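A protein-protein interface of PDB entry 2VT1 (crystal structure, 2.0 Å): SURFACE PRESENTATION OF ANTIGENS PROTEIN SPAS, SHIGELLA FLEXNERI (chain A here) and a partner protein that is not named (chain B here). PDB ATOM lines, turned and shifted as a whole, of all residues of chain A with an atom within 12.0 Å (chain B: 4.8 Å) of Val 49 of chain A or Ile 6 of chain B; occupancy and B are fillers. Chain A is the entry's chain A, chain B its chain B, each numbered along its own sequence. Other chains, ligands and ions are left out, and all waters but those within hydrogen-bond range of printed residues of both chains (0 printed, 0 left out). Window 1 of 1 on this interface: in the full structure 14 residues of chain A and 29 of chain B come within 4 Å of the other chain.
The backbone NH of Lys 47 of chain A lies within hydrogen-bond range of the backbone carbonyl oxygen of Ile 8 of chain B, 2.7 Å away. O of Leu 48 of chain A lies within hydrogen-bond range of N of Ile 8 of chain B (2.9 Å). N of Val 49 of chain A is in hydrogen-bond range of O of Pro 42 of chain B (3.0 Å). N of Val 44 of chain B lies within hydrogen-bond range of O of Val 49 of chain A. N of Val 50 of chain A sits at hydrogen-bond distance from O of Ile 6 of chain B, at 2.6 Å. N of Met 51 of chain A sits at hydrogen-bond distance from O of Val 44 of chain B, 3.0 Å away. The side-chain amide oxygen (OD1) of Asn 52 of chain A sits at hydrogen-bond distance from the backbone NH (N) of Ile 4 of chain B, at 3.0 Å.
The backbone carbonyl oxygen (O) of Asp 42 of chain A sits at hydrogen-bond distance from the side-chain hydroxyl (OG) of Ser 46 of chain A (2.8 Å). N of Gly 7 of chain B lies within hydrogen-bond range of O of Leu 22 of chain B (3.0 Å). The backbone carbonyl oxygen of Ala 36 of chain B sits at hydrogen-bond distance from the backbone NH of Ile 41 of chain B.
Ile 43 of chain A touches Leu 22 of chain B (CG1 to CD2, 3.4 Å). Val 32 of chain B touches Ile 43 of chain A. CA of Ala 36 of chain B touches CG2 of Ile 43 of chain A, 3.8 Å away. Ser 46 of chain A touches Ile 41 of chain B (O to CD1, 3.7 Å). Gly 7 of chain B touches Leu 48 of chain A (CA to O, 3.7 Å). Pro 42 of chain B touches Leu 48 of chain A (O to CA, 3.5 Å). O of Val 50 of chain A touches O of Ile 4 of chain B, at 3.9 Å. Val 50 of chain A touches Ala 5 of chain B. O of Val 44 of chain B touches CA of Val 50 of chain A, 3.5 Å away. Met 51 of chain A touches Thr 43 of chain B (CE to OG1, 3.6 Å).
Asn 45 of chain A touches none of the printed residues of chain B. Printed residues of chain B within 4 Å of Lys 47 of chain A: Ile 8 (2.7 Å) and Pro 42 (3.4 Å). Of the printed residues of chain B, Leu 48 of chain A touches Gly 7, Ile 8 and Pro 42. Val 49 of chain A touches just these residues of chain B: Ile 6, Pro 42, Thr 43 and Val 44. Ile 4 of chain B touches three residues of chain A. Ala 5 of chain B touches just one residue of chain A: Val 50. Printed residues of chain A within 4 Å of Ile 6 of chain B: Val 49 (3.3 Å) and Val 50 (2.6 Å). No residue of chain A comes within 4 Å of Ile 20 of chain B. Leu 22 of chain B touches just one residue of chain A: Ile 43. Val 32 of chain B touches just one residue of chain A: Ile 43. Ala 36 of chain B touches just one residue of chain A: Ile 43 (3.8 Å). Of chain A, only Lys 47, Leu 48 and Val 49 come within 4 Å of Pro 42 of chain B. Thr 43 of chain B touches just these residues of chain A: Val 49 (3.4 Å) and Met 51 (3.6 Å). Printed residues of chain A within 4 Å of Val 44 of chain B: Val 49 (3.0 Å), Val 50 (3.5 Å) and Met 51 (3.0 Å). No residue of chain A comes within 4 Å of Leu 53 of chain B. The nearest printed residue of chain B that does not touch Val 49 of chain A is Ala 5 of chain B (4.1 Å). The nearest printed residue of chain B that does not touch Leu 48 of chain A is Ile 6 of chain B (4.01 Å).
Hydrophobic or aromatic side chains of chain B that line the printed part of chain A: Ile 4, Ile 8, Leu 22, Val 32, Ala 36, Ile 41, Pro 42 and Ala 50. Printed residues of chain A that touch a printed residue of chain B: Ile 43, Ser 46, Lys 47, Leu 48, Val 49, Val 50, Met 51 and Asn 52. Hydrophobic or aromatic side chains of chain A that line the printed part of chain B: Ile 43, Leu 48, Val 49, Val 50 and Met 51. Among the printed residues, 26 pairs touch across the chains.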
ATOM      1  N   LEU A  35     -21.826  30.714   9.179  1.00  0.00           N
ATOM      2  CA  LEU A  35     -22.796  30.570  10.252  1.00  0.00           C
ATOM      3  C   LEU A  35     -24.180  31.091   9.861  1.00  0.00           C
ATOM      4  O   LEU A  35     -24.308  32.120   9.206  1.00  0.00           O
ATOM      5  CB  LEU A  35     -22.318  31.343  11.481  1.00  0.00           C
ATOM      6  CG  LEU A  35     -20.968  30.945  12.071  1.00  0.00           C
ATOM      7  CD1 LEU A  35     -20.680  31.866  13.226  1.00  0.00           C
ATOM      8  CD2 LEU A  35     -20.934  29.478  12.503  1.00  0.00           C
ATOM      9  N   GLN A  38     -29.287  32.254  13.259  1.00  0.00           N
ATOM     10  CA  GLN A  38     -29.616  31.825  14.617  1.00  0.00           C
ATOM     11  C   GLN A  38     -28.373  31.517  15.437  1.00  0.00           C
ATOM     12  O   GLN A  38     -28.323  31.818  16.610  1.00  0.00           O
ATOM     13  CB  GLN A  38     -30.532  30.605  14.591  1.00  0.00           C
ATOM     14  CG  GLN A  38     -30.983  30.152  15.942  1.00  0.00           C
ATOM     15  CD  GLN A  38     -31.868  31.143  16.623  1.00  0.00           C
ATOM     16  OE1 GLN A  38     -32.711  31.795  15.990  1.00  0.00           O
ATOM     17  NE2 GLN A  38     -31.687  31.279  17.927  1.00  0.00           N
ATOM     18  N   THR A  39     -27.362  30.922  14.819  1.00  0.00           N
ATOM     19  CA  THR A  39     -26.101  30.639  15.526  1.00  0.00           C
ATOM     20  C   THR A  39     -25.373  31.952  15.877  1.00  0.00           C
ATOM     21  O   THR A  39     -24.808  32.087  16.971  1.00  0.00           O
ATOM     22  CB  THR A  39     -25.192  29.648  14.724  1.00  0.00           C
ATOM     23  OG1 THR A  39     -25.859  28.380  14.587  1.00  0.00           O
ATOM     24  CG2 THR A  39     -23.834  29.428  15.415  1.00  0.00           C
ATOM     25  N   LYS A  40     -25.413  32.928  14.968  1.00  0.00           N
ATOM     26  CA  LYS A  40     -24.797  34.232  15.218  1.00  0.00           C
ATOM     27  C   LYS A  40     -25.447  34.912  16.419  1.00  0.00           C
ATOM     28  O   LYS A  40     -24.766  35.462  17.270  1.00  0.00           O
ATOM     29  CB  LYS A  40     -24.904  35.125  13.981  1.00  0.00           C
ATOM     30  CG  LYS A  40     -23.909  34.782  12.867  1.00  0.00           C
ATOM     31  CD  LYS A  40     -24.018  35.837  11.812  1.00  0.00           C
ATOM     32  CE  LYS A  40     -23.365  35.482  10.537  1.00  0.00           C
ATOM     33  NZ  LYS A  40     -23.905  36.381   9.485  1.00  0.00           N
ATOM     34  N   SER A  41     -26.776  34.849  16.470  1.00  0.00           N
ATOM     35  CA  SER A  41     -27.567  35.380  17.569  1.00  0.00           C
ATOM     36  C   SER A  41     -27.258  34.687  18.886  1.00  0.00           C
ATOM     37  O   SER A  41     -27.110  35.352  19.907  1.00  0.00           O
ATOM     38  CB  SER A  41     -29.053  35.234  17.232  1.00  0.00           C
ATOM     39  OG  SER A  41     -29.860  35.597  18.337  1.00  0.00           O
ATOM     40  N   ASP A  42     -27.148  33.355  18.864  1.00  0.00           N
ATOM     41  CA  ASP A  42     -26.802  32.573  20.057  1.00  0.00           C
ATOM     42  C   ASP A  42     -25.458  32.997  20.641  1.00  0.00           C
ATOM     43  O   ASP A  42     -25.329  33.126  21.862  1.00  0.00           O
ATOM     44  CB  ASP A  42     -26.766  31.088  19.738  1.00  0.00           C
ATOM     45  CG  ASP A  42     -28.142  30.508  19.492  1.00  0.00           C
ATOM     46  OD1 ASP A  42     -29.142  31.201  19.757  1.00  0.00           O
ATOM     47  OD2 ASP A  42     -28.233  29.351  19.038  1.00  0.00           O
ATOM     48  N   ILE A  43     -24.473  33.208  19.767  1.00  0.00           N
ATOM     49  CA  ILE A  43     -23.136  33.728  20.133  1.00  0.00           C
ATOM     50  C   ILE A  43     -23.215  35.131  20.735  1.00  0.00           C
ATOM     51  O   ILE A  43     -22.619  35.408  21.782  1.00  0.00           O
ATOM     52  CB  ILE A  43     -22.166  33.765  18.897  1.00  0.00           C
ATOM     53  CG1 ILE A  43     -21.921  32.369  18.343  1.00  0.00           C
ATOM     54  CG2 ILE A  43     -20.787  34.399  19.259  1.00  0.00           C
ATOM     55  CD1 ILE A  43     -21.197  32.347  17.036  1.00  0.00           C
ATOM     56  N   ARG A  44     -23.946  36.021  20.069  1.00  0.00           N
ATOM     57  CA  ARG A  44     -24.125  37.380  20.556  1.00  0.00           C
ATOM     58  C   ARG A  44     -24.836  37.397  21.913  1.00  0.00           C
ATOM     59  O   ARG A  44     -24.657  38.323  22.716  1.00  0.00           O
ATOM     60  CB  ARG A  44     -24.932  38.221  19.550  1.00  0.00           C
ATOM     61  CG  ARG A  44     -24.164  38.634  18.319  1.00  0.00           C
ATOM     62  CD  ARG A  44     -24.886  39.728  17.548  1.00  0.00           C
ATOM     63  NE  ARG A  44     -26.273  39.366  17.271  1.00  0.00           N
ATOM     64  CZ  ARG A  44     -26.709  38.834  16.130  1.00  0.00           C
ATOM     65  NH1 ARG A  44     -25.878  38.584  15.130  1.00  0.00           N
ATOM     66  NH2 ARG A  44     -27.989  38.540  15.998  1.00  0.00           N
ATOM     67  N   ASN A  45     -25.638  36.366  22.172  1.00  0.00           N
ATOM     68  CA  ASN A  45     -26.411  36.308  23.401  1.00  0.00           C
ATOM     69  C   ASN A  45     -25.770  35.516  24.523  1.00  0.00           C
ATOM     70  O   ASN A  45     -26.413  35.279  25.527  1.00  0.00           O
ATOM     71  CB  ASN A  45     -27.796  35.758  23.119  1.00  0.00           C
ATOM     72  CG  ASN A  45     -28.716  36.807  22.610  1.00  0.00           C
ATOM     73  OD1 ASN A  45     -29.396  37.459  23.386  1.00  0.00           O
ATOM     74  ND2 ASN A  45     -28.718  37.017  21.311  1.00  0.00           N
ATOM     75  N   SER A  46     -24.511  35.126  24.343  1.00  0.00           N
ATOM     76  CA  SER A  46     -23.754  34.359  25.340  1.00  0.00           C
ATOM     77  C   SER A  46     -22.803  35.267  26.137  1.00  0.00           C
ATOM     78  O   SER A  46     -22.452  36.359  25.681  1.00  0.00           O
ATOM     79  CB  SER A  46     -22.922  33.271  24.652  1.00  0.00           C
ATOM     80  OG  SER A  46     -23.740  32.337  23.987  1.00  0.00           O
ATOM     81  N   LYS A  47     -22.398  34.820  27.333  1.00  0.00           N
ATOM     82  CA  LYS A  47     -21.410  35.563  28.134  1.00  0.00           C
ATOM     83  C   LYS A  47     -20.009  35.168  27.693  1.00  0.00           C
ATOM     84  O   LYS A  47     -19.089  35.980  27.727  1.00  0.00           O
ATOM     85  CB  LYS A  47     -21.574  35.284  29.640  1.00  0.00           C
ATOM     86  CG  LYS A  47     -22.899  35.747  30.223  1.00  0.00           C
ATOM     87  CD  LYS A  47     -23.141  37.235  29.961  1.00  0.00           C
ATOM     88  CE  LYS A  47     -24.558  37.644  30.354  1.00  0.00           C
ATOM     89  NZ  LYS A  47     -24.682  39.109  30.598  1.00  0.00           N
ATOM     90  N   LEU A  48     -19.865  33.902  27.307  1.00  0.00           N
ATOM     91  CA  LEU A  48     -18.597  33.367  26.775  1.00  0.00           C
ATOM     92  C   LEU A  48     -18.790  32.129  25.909  1.00  0.00           C
ATOM     93  O   LEU A  48     -19.849  31.506  25.909  1.00  0.00           O
ATOM     94  CB  LEU A  48     -17.654  32.997  27.916  1.00  0.00           C
ATOM     95  CG  LEU A  48     -18.074  31.834  28.821  1.00  0.00           C
ATOM     96  CD1 LEU A  48     -16.848  31.174  29.437  1.00  0.00           C
ATOM     97  CD2 LEU A  48     -19.008  32.333  29.892  1.00  0.00           C
ATOM     98  N   VAL A  49     -17.744  31.770  25.173  1.00  0.00           N
ATOM     99  CA  VAL A  49     -17.729  30.534  24.441  1.00  0.00           C
ATOM    100  C   VAL A  49     -16.591  29.745  25.014  1.00  0.00           C
ATOM    101  O   VAL A  49     -15.487  30.254  25.083  1.00  0.00           O
ATOM    102  CB  VAL A  49     -17.495  30.750  22.935  1.00  0.00           C
ATOM    103  CG1 VAL A  49     -17.211  29.444  22.235  1.00  0.00           C
ATOM    104  CG2 VAL A  49     -18.694  31.443  22.309  1.00  0.00           C
ATOM    105  N   VAL A  50     -16.860  28.512  25.436  1.00  0.00           N
ATOM    106  CA  VAL A  50     -15.810  27.624  25.915  1.00  0.00           C
ATOM    107  C   VAL A  50     -15.320  26.728  24.780  1.00  0.00           C
ATOM    108  O   VAL A  50     -16.115  26.115  24.066  1.00  0.00           O
ATOM    109  CB  VAL A  50     -16.302  26.730  27.060  1.00  0.00           C
ATOM    110  CG1 VAL A  50     -15.159  25.844  27.567  1.00  0.00           C
ATOM    111  CG2 VAL A  50     -16.880  27.572  28.188  1.00  0.00           C
ATOM    112  N   MET A  51     -14.006  26.645  24.627  1.00  0.00           N
ATOM    113  CA  MET A  51     -13.423  25.861  23.566  1.00  0.00           C
ATOM    114  C   MET A  51     -12.366  24.901  24.061  1.00  0.00           C
ATOM    115  O   MET A  51     -11.823  25.046  25.150  1.00  0.00           O
ATOM    116  CB  MET A  51     -12.830  26.763  22.491  1.00  0.00           C
ATOM    117  CG  MET A  51     -12.567  28.167  22.947  1.00  0.00           C
ATOM    118  SD  MET A  51     -11.759  29.099  21.647  1.00  0.00           S
ATOM    119  CE  MET A  51     -10.407  29.903  22.523  1.00  0.00           C
ATOM    120  N   ASN A  52     -12.104  23.886  23.257  1.00  0.00           N
ATOM    121  CA  ASN A  52     -10.972  23.049  23.518  1.00  0.00           C
ATOM    122  C   ASN A  52      -9.802  23.628  22.758  1.00  0.00           C
ATOM    123  O   ASN A  52      -8.825  22.938  22.447  1.00  0.00           O
ATOM    124  CB  ASN A  52     -11.260  21.571  23.193  1.00  0.00           C
ATOM    125  CG  ASN A  52     -11.519  21.302  21.711  1.00  0.00           C
ATOM    126  OD1 ASN A  52     -11.695  22.206  20.896  1.00  0.00           O
ATOM    127  ND2 ASN A  52     -11.552  20.020  21.370  1.00  0.00           N
ATOM    128  OXT ASN A  52      -9.825  24.833  22.465  1.00  0.00           O
ATOM    129  N   ILE B   4     -14.251  21.824  19.437  1.00  0.00           N
ATOM    130  CA  ILE B   4     -15.507  21.979  20.178  1.00  0.00           C
ATOM    131  C   ILE B   4     -15.735  23.464  20.558  1.00  0.00           C
ATOM    132  O   ILE B   4     -14.808  24.177  20.934  1.00  0.00           O
ATOM    133  CB  ILE B   4     -15.507  21.124  21.473  1.00  0.00           C
ATOM    134  CG1 ILE B   4     -15.434  19.629  21.157  1.00  0.00           C
ATOM    135  CG2 ILE B   4     -16.744  21.416  22.302  1.00  0.00           C
ATOM    136  CD1 ILE B   4     -15.034  18.777  22.345  1.00  0.00           C
ATOM    137  N   ALA B   5     -16.972  23.925  20.433  1.00  0.00           N
ATOM    138  CA  ALA B   5     -17.351  25.250  20.904  1.00  0.00           C
ATOM    139  C   ALA B   5     -18.645  25.116  21.698  1.00  0.00           C
ATOM    140  O   ALA B   5     -19.622  24.573  21.198  1.00  0.00           O
ATOM    141  CB  ALA B   5     -17.544  26.194  19.733  1.00  0.00           C
ATOM    142  N   ILE B   6     -18.635  25.583  22.942  1.00  0.00           N
ATOM    143  CA  ILE B   6     -19.842  25.574  23.778  1.00  0.00           C
ATOM    144  C   ILE B   6     -20.108  27.009  24.221  1.00  0.00           C
ATOM    145  O   ILE B   6     -19.265  27.677  24.859  1.00  0.00           O
ATOM    146  CB  ILE B   6     -19.723  24.647  25.037  1.00  0.00           C
ATOM    147  CG1 ILE B   6     -19.016  23.314  24.719  1.00  0.00           C
ATOM    148  CG2 ILE B   6     -21.108  24.441  25.699  1.00  0.00           C
ATOM    149  CD1 ILE B   6     -19.857  22.200  24.052  1.00  0.00           C
ATOM    150  N   GLY B   7     -21.279  27.493  23.845  1.00  0.00           N
ATOM    151  CA  GLY B   7     -21.703  28.809  24.211  1.00  0.00           C
ATOM    152  C   GLY B   7     -22.324  28.740  25.587  1.00  0.00           C
ATOM    153  O   GLY B   7     -23.038  27.790  25.895  1.00  0.00           O
ATOM    154  N   ILE B   8     -22.042  29.740  26.413  1.00  0.00           N
ATOM    155  CA  ILE B   8     -22.564  29.788  27.780  1.00  0.00           C
ATOM    156  C   ILE B   8     -23.246  31.121  28.085  1.00  0.00           C
ATOM    157  O   ILE B   8     -22.678  32.198  27.924  1.00  0.00           O
ATOM    158  CB  ILE B   8     -21.472  29.538  28.832  1.00  0.00           C
ATOM    159  CG1 ILE B   8     -20.757  28.218  28.576  1.00  0.00           C
ATOM    160  CG2 ILE B   8     -22.075  29.532  30.226  1.00  0.00           C
ATOM    161  CD1 ILE B   8     -21.557  27.015  28.905  1.00  0.00           C
ATOM    162  N   ILE B  20     -26.412  26.365  28.344  1.00  0.00           N
ATOM    163  CA  ILE B  20     -25.709  26.108  27.081  1.00  0.00           C
ATOM    164  C   ILE B  20     -26.529  26.584  25.877  1.00  0.00           C
ATOM    165  O   ILE B  20     -27.584  26.029  25.589  1.00  0.00           O
ATOM    166  CB  ILE B  20     -25.388  24.605  26.903  1.00  0.00           C
ATOM    167  CG1 ILE B  20     -24.362  24.151  27.954  1.00  0.00           C
ATOM    168  CG2 ILE B  20     -24.899  24.334  25.448  1.00  0.00           C
ATOM    169  CD1 ILE B  20     -24.206  22.647  28.078  1.00  0.00           C
ATOM    170  N   LEU B  22     -25.183  26.938  22.619  1.00  0.00           N
ATOM    171  CA  LEU B  22     -24.741  26.362  21.366  1.00  0.00           C
ATOM    172  C   LEU B  22     -23.713  25.280  21.641  1.00  0.00           C
ATOM    173  O   LEU B  22     -22.962  25.337  22.614  1.00  0.00           O
ATOM    174  CB  LEU B  22     -24.207  27.453  20.406  1.00  0.00           C
ATOM    175  CG  LEU B  22     -22.815  28.091  20.566  1.00  0.00           C
ATOM    176  CD1 LEU B  22     -21.740  27.255  19.894  1.00  0.00           C
ATOM    177  CD2 LEU B  22     -22.807  29.478  19.977  1.00  0.00           C
ATOM    178  N   ILE B  23     -23.732  24.266  20.804  1.00  0.00           N
ATOM    179  CA  ILE B  23     -22.687  23.267  20.792  1.00  0.00           C
ATOM    180  C   ILE B  23     -22.353  22.976  19.345  1.00  0.00           C
ATOM    181  O   ILE B  23     -23.189  22.461  18.607  1.00  0.00           O
ATOM    182  CB  ILE B  23     -23.107  21.947  21.448  1.00  0.00           C
ATOM    183  CG1 ILE B  23     -23.563  22.170  22.900  1.00  0.00           C
ATOM    184  CG2 ILE B  23     -21.940  20.954  21.393  1.00  0.00           C
ATOM    185  CD1 ILE B  23     -23.825  20.879  23.680  1.00  0.00           C
ATOM    186  N   VAL B  32     -17.463  29.572  14.811  1.00  0.00           N
ATOM    187  CA  VAL B  32     -18.025  30.143  16.035  1.00  0.00           C
ATOM    188  C   VAL B  32     -16.955  30.949  16.794  1.00  0.00           C
ATOM    189  O   VAL B  32     -17.205  32.059  17.255  1.00  0.00           O
ATOM    190  CB  VAL B  32     -18.631  29.058  16.937  1.00  0.00           C
ATOM    191  CG1 VAL B  32     -18.988  29.640  18.279  1.00  0.00           C
ATOM    192  CG2 VAL B  32     -19.879  28.460  16.286  1.00  0.00           C
ATOM    193  N   ALA B  36     -17.222  34.958  17.409  1.00  0.00           N
ATOM    194  CA  ALA B  36     -17.194  35.376  18.802  1.00  0.00           C
ATOM    195  C   ALA B  36     -16.114  36.431  19.033  1.00  0.00           C
ATOM    196  O   ALA B  36     -16.363  37.451  19.655  1.00  0.00           O
ATOM    197  CB  ALA B  36     -16.973  34.163  19.720  1.00  0.00           C
ATOM    198  N   ILE B  41     -17.145  38.672  22.079  1.00  0.00           N
ATOM    199  CA  ILE B  41     -17.522  37.665  23.045  1.00  0.00           C
ATOM    200  C   ILE B  41     -16.269  36.880  23.424  1.00  0.00           C
ATOM    201  O   ILE B  41     -15.630  36.283  22.575  1.00  0.00           O
ATOM    202  CB  ILE B  41     -18.542  36.698  22.434  1.00  0.00           C
ATOM    203  CG1 ILE B  41     -19.824  37.447  22.006  1.00  0.00           C
ATOM    204  CG2 ILE B  41     -18.784  35.528  23.359  1.00  0.00           C
ATOM    205  CD1 ILE B  41     -20.558  38.164  23.130  1.00  0.00           C
ATOM    206  N   PRO B  42     -15.907  36.880  24.707  1.00  0.00           N
ATOM    207  CA  PRO B  42     -14.713  36.173  25.181  1.00  0.00           C
ATOM    208  C   PRO B  42     -14.719  34.695  24.826  1.00  0.00           C
ATOM    209  O   PRO B  42     -15.749  34.034  24.937  1.00  0.00           O
ATOM    210  CB  PRO B  42     -14.786  36.324  26.705  1.00  0.00           C
ATOM    211  CG  PRO B  42     -15.686  37.440  26.957  1.00  0.00           C
ATOM    212  CD  PRO B  42     -16.663  37.486  25.811  1.00  0.00           C
ATOM    213  N   THR B  43     -13.577  34.186  24.385  1.00  0.00           N
ATOM    214  CA  THR B  43     -13.447  32.793  24.097  1.00  0.00           C
ATOM    215  C   THR B  43     -12.375  32.250  25.007  1.00  0.00           C
ATOM    216  O   THR B  43     -11.239  32.713  24.992  1.00  0.00           O
ATOM    217  CB  THR B  43     -13.091  32.509  22.614  1.00  0.00           C
ATOM    218  OG1 THR B  43     -11.877  33.180  22.245  1.00  0.00           O
ATOM    219  CG2 THR B  43     -14.213  32.935  21.706  1.00  0.00           C
ATOM    220  N   VAL B  44     -12.744  31.256  25.792  1.00  0.00           N
ATOM    221  CA  VAL B  44     -11.886  30.756  26.834  1.00  0.00           C
ATOM    222  C   VAL B  44     -11.578  29.299  26.566  1.00  0.00           C
ATOM    223  O   VAL B  44     -12.481  28.497  26.370  1.00  0.00           O
ATOM    224  CB  VAL B  44     -12.581  30.859  28.198  1.00  0.00           C
ATOM    225  CG1 VAL B  44     -11.666  30.334  29.289  1.00  0.00           C
ATOM    226  CG2 VAL B  44     -13.007  32.307  28.486  1.00  0.00           C
ATOM    227  N   ALA B  50     -14.684  21.562  27.925  1.00  0.00           N
ATOM    228  CA  ALA B  50     -15.280  21.521  26.603  1.00  0.00           C
ATOM    229  C   ALA B  50     -15.733  20.094  26.245  1.00  0.00           C
ATOM    230  O   ALA B  50     -16.881  19.872  25.848  1.00  0.00           O
ATOM    231  CB  ALA B  50     -14.290  22.051  25.592  1.00  0.00           C
ATOM    232  N   LEU B  53     -18.722  18.720  28.571  1.00  0.00           N
ATOM    233  CA  LEU B  53     -20.037  19.269  28.266  1.00  0.00           C
ATOM    234  C   LEU B  53     -20.524  18.700  26.954  1.00  0.00           C
ATOM    235  O   LEU B  53     -21.694  18.367  26.805  1.00  0.00           O
ATOM    236  CB  LEU B  53     -19.988  20.804  28.212  1.00  0.00           C
ATOM    237  CG  LEU B  53     -19.591  21.514  29.509  1.00  0.00           C
ATOM    238  CD1 LEU B  53     -19.459  23.031  29.299  1.00  0.00           C
ATOM    239  CD2 LEU B  53     -20.595  21.204  30.628  1.00  0.00           C
ATOM    240  N   TYR B  54     -19.617  18.564  25.999  1.00  0.00           N
ATOM    241  CA  TYR B  54     -19.980  17.989  24.718  1.00  0.00           C
ATOM    242  C   TYR B  54     -20.466  16.544  24.867  1.00  0.00           C
ATOM    243  O   TYR B  54     -21.402  16.121  24.163  1.00  0.00           O
ATOM    244  CB  TYR B  54     -18.795  18.038  23.757  1.00  0.00           C
ATOM    245  CG  TYR B  54     -19.079  17.314  22.466  1.00  0.00           C
ATOM    246  CD1 TYR B  54     -18.470  16.111  22.181  1.00  0.00           C
ATOM    247  CD2 TYR B  54     -19.994  17.817  21.561  1.00  0.00           C
ATOM    248  CE1 TYR B  54     -18.743  15.440  21.017  1.00  0.00           C
ATOM    249  CE2 TYR B  54     -20.263  17.164  20.402  1.00  0.00           C
ATOM    250  CZ  TYR B  54     -19.643  15.973  20.135  1.00  0.00           C
ATOM    251  OH  TYR B  54     -19.924  15.307  18.969  1.00  0.00           O
